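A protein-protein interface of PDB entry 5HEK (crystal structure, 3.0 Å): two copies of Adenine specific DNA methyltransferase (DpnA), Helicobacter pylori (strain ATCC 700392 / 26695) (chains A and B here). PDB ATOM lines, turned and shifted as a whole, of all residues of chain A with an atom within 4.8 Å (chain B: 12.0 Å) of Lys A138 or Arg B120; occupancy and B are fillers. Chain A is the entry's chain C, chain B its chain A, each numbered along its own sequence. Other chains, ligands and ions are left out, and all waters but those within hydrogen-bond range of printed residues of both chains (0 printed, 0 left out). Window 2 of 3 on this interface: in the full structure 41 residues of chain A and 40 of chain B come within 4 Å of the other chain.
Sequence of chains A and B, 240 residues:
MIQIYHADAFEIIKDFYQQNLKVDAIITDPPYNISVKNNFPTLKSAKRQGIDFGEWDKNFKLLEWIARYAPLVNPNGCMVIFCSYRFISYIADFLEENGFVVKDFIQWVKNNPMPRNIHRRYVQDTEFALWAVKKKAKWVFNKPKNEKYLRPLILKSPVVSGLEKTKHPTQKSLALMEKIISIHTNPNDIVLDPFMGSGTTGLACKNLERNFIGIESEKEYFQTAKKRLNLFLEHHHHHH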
ATOM      1  N   ASN A  76      21.511   2.296   0.846  1.00  0.00           N
ATOM      2  CA  ASN A  76      22.018   2.217  -0.521  1.00  0.00           C
ATOM      3  C   ASN A  76      22.097   0.783  -1.037  1.00  0.00           C
ATOM      4  O   ASN A  76      22.610   0.532  -2.132  1.00  0.00           O
ATOM      5  CB  ASN A  76      23.378   2.890  -0.627  1.00  0.00           C
ATOM      6  CG  ASN A  76      23.304   4.369  -0.337  1.00  0.00           C
ATOM      7  OD1 ASN A  76      22.448   5.071  -0.867  1.00  0.00           O
ATOM      8  ND2 ASN A  76      24.202   4.852   0.508  1.00  0.00           N
ATOM      9  N   TRP A 131      17.230  -8.056 -10.204  1.00  0.00           N
ATOM     10  CA  TRP A 131      18.075  -7.058  -9.552  1.00  0.00           C
ATOM     11  C   TRP A 131      17.253  -5.866  -9.071  1.00  0.00           C
ATOM     12  O   TRP A 131      16.702  -5.110  -9.877  1.00  0.00           O
ATOM     13  CB  TRP A 131      19.166  -6.568 -10.499  1.00  0.00           C
ATOM     14  CG  TRP A 131      19.988  -5.441  -9.922  1.00  0.00           C
ATOM     15  CD1 TRP A 131      20.444  -5.332  -8.640  1.00  0.00           C
ATOM     16  CD2 TRP A 131      20.440  -4.264 -10.611  1.00  0.00           C
ATOM     17  NE1 TRP A 131      21.160  -4.165  -8.494  1.00  0.00           N
ATOM     18  CE2 TRP A 131      21.171  -3.492  -9.690  1.00  0.00           C
ATOM     19  CE3 TRP A 131      20.301  -3.790 -11.923  1.00  0.00           C
ATOM     20  CZ2 TRP A 131      21.763  -2.273 -10.036  1.00  0.00           C
ATOM     21  CZ3 TRP A 131      20.894  -2.578 -12.266  1.00  0.00           C
ATOM     22  CH2 TRP A 131      21.615  -1.834 -11.323  1.00  0.00           C
ATOM     23  N   LYS A 136      15.470   5.031  -2.317  1.00  0.00           N
ATOM     24  CA  LYS A 136      16.199   6.271  -2.547  1.00  0.00           C
ATOM     25  C   LYS A 136      17.696   5.945  -2.646  1.00  0.00           C
ATOM     26  O   LYS A 136      18.549   6.829  -2.681  1.00  0.00           O
ATOM     27  CB  LYS A 136      15.871   7.288  -1.448  1.00  0.00           C
ATOM     28  CG  LYS A 136      16.649   8.621  -1.464  1.00  0.00           C
ATOM     29  CD  LYS A 136      16.502   9.420  -2.767  1.00  0.00           C
ATOM     30  CE  LYS A 136      17.683  10.395  -2.952  1.00  0.00           C
ATOM     31  NZ  LYS A 136      18.460  10.145  -4.204  1.00  0.00           N
ATOM     32  N   ALA A 137      18.015   4.656  -2.705  1.00  0.00           N
ATOM     33  CA  ALA A 137      19.413   4.227  -2.766  1.00  0.00           C
ATOM     34  C   ALA A 137      20.232   4.877  -3.878  1.00  0.00           C
ATOM     35  O   ALA A 137      19.755   5.075  -4.996  1.00  0.00           O
ATOM     36  CB  ALA A 137      19.490   2.715  -2.920  1.00  0.00           C
ATOM     37  N   LYS A 138      21.492   5.153  -3.553  1.00  0.00           N
ATOM     38  CA  LYS A 138      22.497   5.423  -4.555  1.00  0.00           C
ATOM     39  C   LYS A 138      23.212   4.079  -4.673  1.00  0.00           C
ATOM     40  O   LYS A 138      23.976   3.670  -3.791  1.00  0.00           O
ATOM     41  CB  LYS A 138      23.406   6.597  -4.115  1.00  0.00           C
ATOM     42  CG  LYS A 138      24.898   6.369  -4.046  1.00  0.00           C
ATOM     43  CD  LYS A 138      25.644   7.607  -3.533  1.00  0.00           C
ATOM     44  CE  LYS A 138      25.603   7.707  -2.003  1.00  0.00           C
ATOM     45  NZ  LYS A 138      26.172   8.986  -1.473  1.00  0.00           N
ATOM     46  N   TRP A 139      22.933   3.365  -5.757  1.00  0.00           N
ATOM     47  CA  TRP A 139      23.349   1.968  -5.835  1.00  0.00           C
ATOM     48  C   TRP A 139      24.747   1.855  -6.430  1.00  0.00           C
ATOM     49  O   TRP A 139      25.355   2.859  -6.800  1.00  0.00           O
ATOM     50  CB  TRP A 139      22.357   1.130  -6.654  1.00  0.00           C
ATOM     51  CG  TRP A 139      22.198   1.621  -8.061  1.00  0.00           C
ATOM     52  CD1 TRP A 139      22.968   1.293  -9.139  1.00  0.00           C
ATOM     53  CD2 TRP A 139      21.172   2.496  -8.552  1.00  0.00           C
ATOM     54  NE1 TRP A 139      22.510   1.945 -10.260  1.00  0.00           N
ATOM     55  CE2 TRP A 139      21.406   2.686  -9.926  1.00  0.00           C
ATOM     56  CE3 TRP A 139      20.089   3.152  -7.957  1.00  0.00           C
ATOM     57  CZ2 TRP A 139      20.585   3.504 -10.719  1.00  0.00           C
ATOM     58  CZ3 TRP A 139      19.274   3.962  -8.745  1.00  0.00           C
ATOM     59  CH2 TRP A 139      19.529   4.132 -10.106  1.00  0.00           C
ATOM     60  N   VAL A 140      25.238   0.627  -6.544  1.00  0.00           N
ATOM     61  CA  VAL A 140      26.636   0.386  -6.891  1.00  0.00           C
ATOM     62  C   VAL A 140      26.900   0.349  -8.402  1.00  0.00           C
ATOM     63  O   VAL A 140      27.664   1.172  -8.925  1.00  0.00           O
ATOM     64  CB  VAL A 140      27.137  -0.933  -6.260  1.00  0.00           C
ATOM     65  CG1 VAL A 140      28.661  -1.047  -6.376  1.00  0.00           C
ATOM     66  CG2 VAL A 140      26.729  -0.990  -4.808  1.00  0.00           C
ATOM     67  N   PHE A 141      26.285  -0.615  -9.086  1.00  0.00           N
ATOM     68  CA  PHE A 141      26.604  -0.910 -10.488  1.00  0.00           C
ATOM     69  C   PHE A 141      28.094  -1.214 -10.678  1.00  0.00           C
ATOM     70  O   PHE A 141      28.468  -2.367 -10.523  1.00  0.00           O
ATOM     71  CB  PHE A 141      26.147   0.139 -11.490  1.00  0.00           C
ATOM     72  CG  PHE A 141      25.979  -0.457 -12.865  1.00  0.00           C
ATOM     73  CD1 PHE A 141      25.241  -1.625 -13.013  1.00  0.00           C
ATOM     74  CD2 PHE A 141      26.612   0.072 -13.979  1.00  0.00           C
ATOM     75  CE1 PHE A 141      25.100  -2.226 -14.244  1.00  0.00           C
ATOM     76  CE2 PHE A 141      26.471  -0.527 -15.222  1.00  0.00           C
ATOM     77  CZ  PHE A 141      25.718  -1.679 -15.352  1.00  0.00           C
ATOM     78  N   PRO B 115      21.342   3.543 -25.420  1.00  0.00           N
ATOM     79  CA  PRO B 115      21.621   2.372 -24.575  1.00  0.00           C
ATOM     80  C   PRO B 115      20.671   2.018 -23.390  1.00  0.00           C
ATOM     81  O   PRO B 115      20.354   0.827 -23.342  1.00  0.00           O
ATOM     82  CB  PRO B 115      23.013   2.697 -23.998  1.00  0.00           C
ATOM     83  CG  PRO B 115      23.599   3.755 -24.853  1.00  0.00           C
ATOM     84  CD  PRO B 115      22.601   4.150 -25.888  1.00  0.00           C
ATOM     85  N   ARG B 116      20.203   2.910 -22.498  1.00  0.00           N
ATOM     86  CA  ARG B 116      20.492   4.345 -22.425  1.00  0.00           C
ATOM     87  C   ARG B 116      21.669   4.654 -21.474  1.00  0.00           C
ATOM     88  O   ARG B 116      22.771   4.972 -21.924  1.00  0.00           O
ATOM     89  CB  ARG B 116      19.233   5.081 -21.963  1.00  0.00           C
ATOM     90  CG  ARG B 116      18.210   5.247 -23.077  1.00  0.00           C
ATOM     91  CD  ARG B 116      17.184   6.346 -22.835  1.00  0.00           C
ATOM     92  NE  ARG B 116      16.161   6.423 -23.889  1.00  0.00           N
ATOM     93  CZ  ARG B 116      16.385   6.523 -25.202  1.00  0.00           C
ATOM     94  NH1 ARG B 116      17.619   6.590 -25.690  1.00  0.00           N
ATOM     95  NH2 ARG B 116      15.357   6.577 -26.040  1.00  0.00           N
ATOM     96  N   ASN B 117      21.427   4.568 -20.161  1.00  0.00           N
ATOM     97  CA  ASN B 117      22.422   4.955 -19.144  1.00  0.00           C
ATOM     98  C   ASN B 117      23.332   3.797 -18.739  1.00  0.00           C
ATOM     99  O   ASN B 117      22.952   2.946 -17.937  1.00  0.00           O
ATOM    100  CB  ASN B 117      21.713   5.493 -17.894  1.00  0.00           C
ATOM    101  CG  ASN B 117      22.638   6.288 -16.969  1.00  0.00           C
ATOM    102  OD1 ASN B 117      23.865   6.255 -17.100  1.00  0.00           O
ATOM    103  ND2 ASN B 117      22.044   6.999 -16.015  1.00  0.00           N
ATOM    104  N   ILE B 118      24.568   3.815 -19.217  1.00  0.00           N
ATOM    105  CA  ILE B 118      25.411   2.630 -19.103  1.00  0.00           C
ATOM    106  C   ILE B 118      26.328   2.600 -17.886  1.00  0.00           C
ATOM    107  O   ILE B 118      26.872   1.551 -17.543  1.00  0.00           O
ATOM    108  CB  ILE B 118      26.287   2.482 -20.364  1.00  0.00           C
ATOM    109  CG1 ILE B 118      27.043   3.793 -20.640  1.00  0.00           C
ATOM    110  CG2 ILE B 118      25.435   2.103 -21.552  1.00  0.00           C
ATOM    111  CD1 ILE B 118      28.117   3.683 -21.721  1.00  0.00           C
ATOM    112  N   HIS B 119      26.513   3.741 -17.235  1.00  0.00           N
ATOM    113  CA  HIS B 119      27.372   3.771 -16.053  1.00  0.00           C
ATOM    114  C   HIS B 119      26.652   3.411 -14.756  1.00  0.00           C
ATOM    115  O   HIS B 119      27.299   3.058 -13.767  1.00  0.00           O
ATOM    116  CB  HIS B 119      28.034   5.143 -15.914  1.00  0.00           C
ATOM    117  CG  HIS B 119      29.026   5.450 -16.998  1.00  0.00           C
ATOM    118  ND1 HIS B 119      30.140   4.669 -17.223  1.00  0.00           N
ATOM    119  CD2 HIS B 119      29.087   6.461 -17.897  1.00  0.00           C
ATOM    120  CE1 HIS B 119      30.840   5.177 -18.225  1.00  0.00           C
ATOM    121  NE2 HIS B 119      30.223   6.263 -18.651  1.00  0.00           N
ATOM    122  N   ARG B 120      25.332   3.580 -14.726  1.00  0.00           N
ATOM    123  CA  ARG B 120      24.560   3.154 -13.566  1.00  0.00           C
ATOM    124  C   ARG B 120      23.707   1.883 -13.735  1.00  0.00           C
ATOM    125  O   ARG B 120      23.127   1.408 -12.759  1.00  0.00           O
ATOM    126  CB  ARG B 120      23.676   4.317 -13.127  1.00  0.00           C
ATOM    127  CG  ARG B 120      24.500   5.565 -12.809  1.00  0.00           C
ATOM    128  CD  ARG B 120      25.254   5.376 -11.511  1.00  0.00           C
ATOM    129  NE  ARG B 120      24.303   5.267 -10.422  1.00  0.00           N
ATOM    130  CZ  ARG B 120      24.454   4.429  -9.410  1.00  0.00           C
ATOM    131  NH1 ARG B 120      25.508   3.626  -9.382  1.00  0.00           N
ATOM    132  NH2 ARG B 120      23.544   4.368  -8.447  1.00  0.00           N
ATOM    133  N   ARG B 121      23.636   1.321 -14.942  1.00  0.00           N
ATOM    134  CA  ARG B 121      22.624   0.284 -15.209  1.00  0.00           C
ATOM    135  C   ARG B 121      22.934  -0.615 -16.419  1.00  0.00           C
ATOM    136  O   ARG B 121      23.769  -0.272 -17.262  1.00  0.00           O
ATOM    137  CB  ARG B 121      21.261   0.975 -15.391  1.00  0.00           C
ATOM    138  CG  ARG B 121      20.031   0.090 -15.299  1.00  0.00           C
ATOM    139  CD  ARG B 121      18.762   0.943 -15.318  1.00  0.00           C
ATOM    140  NE  ARG B 121      17.533   0.145 -15.301  1.00  0.00           N
ATOM    141  CZ  ARG B 121      16.317   0.647 -15.091  1.00  0.00           C
ATOM    142  NH1 ARG B 121      16.159   1.943 -14.853  1.00  0.00           N
ATOM    143  NH2 ARG B 121      15.259  -0.150 -15.096  1.00  0.00           N
ATOM    144  N   TYR B 122      22.285  -1.775 -16.492  1.00  0.00           N
ATOM    145  CA  TYR B 122      22.401  -2.635 -17.668  1.00  0.00           C
ATOM    146  C   TYR B 122      21.660  -1.972 -18.821  1.00  0.00           C
ATOM    147  O   TYR B 122      20.757  -1.175 -18.591  1.00  0.00           O
ATOM    148  CB  TYR B 122      21.818  -4.039 -17.421  1.00  0.00           C
ATOM    149  CG  TYR B 122      22.503  -4.850 -16.334  1.00  0.00           C
ATOM    150  CD1 TYR B 122      23.670  -5.559 -16.591  1.00  0.00           C
ATOM    151  CD2 TYR B 122      21.942  -4.955 -15.067  1.00  0.00           C
ATOM    152  CE1 TYR B 122      24.284  -6.307 -15.615  1.00  0.00           C
ATOM    153  CE2 TYR B 122      22.544  -5.697 -14.088  1.00  0.00           C
ATOM    154  CZ  TYR B 122      23.716  -6.374 -14.368  1.00  0.00           C
ATOM    155  OH  TYR B 122      24.328  -7.124 -13.388  1.00  0.00           O
ATOM    156  N   VAL B 123      22.056  -2.256 -20.057  1.00  0.00           N
ATOM    157  CA  VAL B 123      21.227  -1.890 -21.211  1.00  0.00           C
ATOM    158  C   VAL B 123      20.158  -2.956 -21.433  1.00  0.00           C
ATOM    159  O   VAL B 123      20.424  -4.145 -21.243  1.00  0.00           O
ATOM    160  CB  VAL B 123      22.048  -1.740 -22.503  1.00  0.00           C
ATOM    161  CG1 VAL B 123      23.004  -0.581 -22.362  1.00  0.00           C
ATOM    162  CG2 VAL B 123      22.816  -3.017 -22.812  1.00  0.00           C
ATOM    163  N   GLN B 124      18.948  -2.569 -21.821  1.00  0.00           N
ATOM    164  CA  GLN B 124      17.963  -3.610 -22.080  1.00  0.00           C
ATOM    165  C   GLN B 124      18.057  -3.939 -23.567  1.00  0.00           C
ATOM    166  O   GLN B 124      17.567  -3.200 -24.427  1.00  0.00           O
ATOM    167  CB  GLN B 124      16.549  -3.160 -21.689  1.00  0.00           C
ATOM    168  CG  GLN B 124      16.395  -2.688 -20.235  1.00  0.00           C
ATOM    169  CD  GLN B 124      16.823  -1.241 -20.014  1.00  0.00           C
ATOM    170  OE1 GLN B 124      17.482  -0.635 -20.863  1.00  0.00           O
ATOM    171  NE2 GLN B 124      16.459  -0.686 -18.859  1.00  0.00           N
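The backbone carbonyl oxygen (O) of Arg B120 lies within hydrogen-bond range of the indole nitrogen (NE1) of Trp A139 (2.6 Å).
O of Val A140 is in hydrogen-bond range of NH1 of Arg B120 (3.3 Å).
OD1 of Asn A76 is in hydrogen-bond range of N of Lys A138 (2.9 Å).
Among the printed residues, pairs that only touch across the chains: Phe A141 with Arg B121 (3.1 Å), Phe A141 with His B119 (3.1 Å), Phe A141 with Ile B118 (3.1 Å), Phe A141 with Arg B120 (3.4 Å), Phe A141 with Tyr B122 (3.6 Å), Trp A131 with Tyr B122 (3.7 Å), Lys A138 with Arg B120 (3.8 Å) and Trp A131 with Arg B120 (3.9 Å).
Lys A138 touches one residue of chain B.
Arg B120 touches just these residues of chain A: Trp A131 (3.9 Å), Lys A138 (3.8 Å), Trp A139 (2.6 Å), Val A140 (3.3 Å) and Phe A141 (3.4 Å).
No residue of chain B comes within 4 Å of Asn A76.
No residue of chain B comes within 4 Å of Ala A137.
Trp A139 touches just one residue of chain B: Arg B120 (2.6 Å).
Val A140 touches one residue of chain B.
Printed residues of chain B within 4 Å of Trp A131: Arg B120 and Tyr B122.
Of the printed residues of chain A, Tyr B122 touches Trp A131 (3.7 Å) and Phe A141 (3.6 Å).
Printed residues of chain A within 4 Å of His B119: Phe A141.
Of the printed residues of chain A, Arg B121 touches Phe A141 (3.1 Å).
Of the 8 printed residues of chain A, 5 touch a printed residue of chain B.
Hydrophobic or aromatic side chains of chain A within 4 Å of the printed part of chain B: Trp A131, Trp A139 and Phe A141.
Hydrophobic or aromatic side chains of chain B that line the printed part of chain A: Tyr B122.
Among the printed residues, no Asp or Glu carboxylate lies within 4 Å of a Lys or Arg side-chain nitrogen of the other chain.
No position is printed for both chains.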
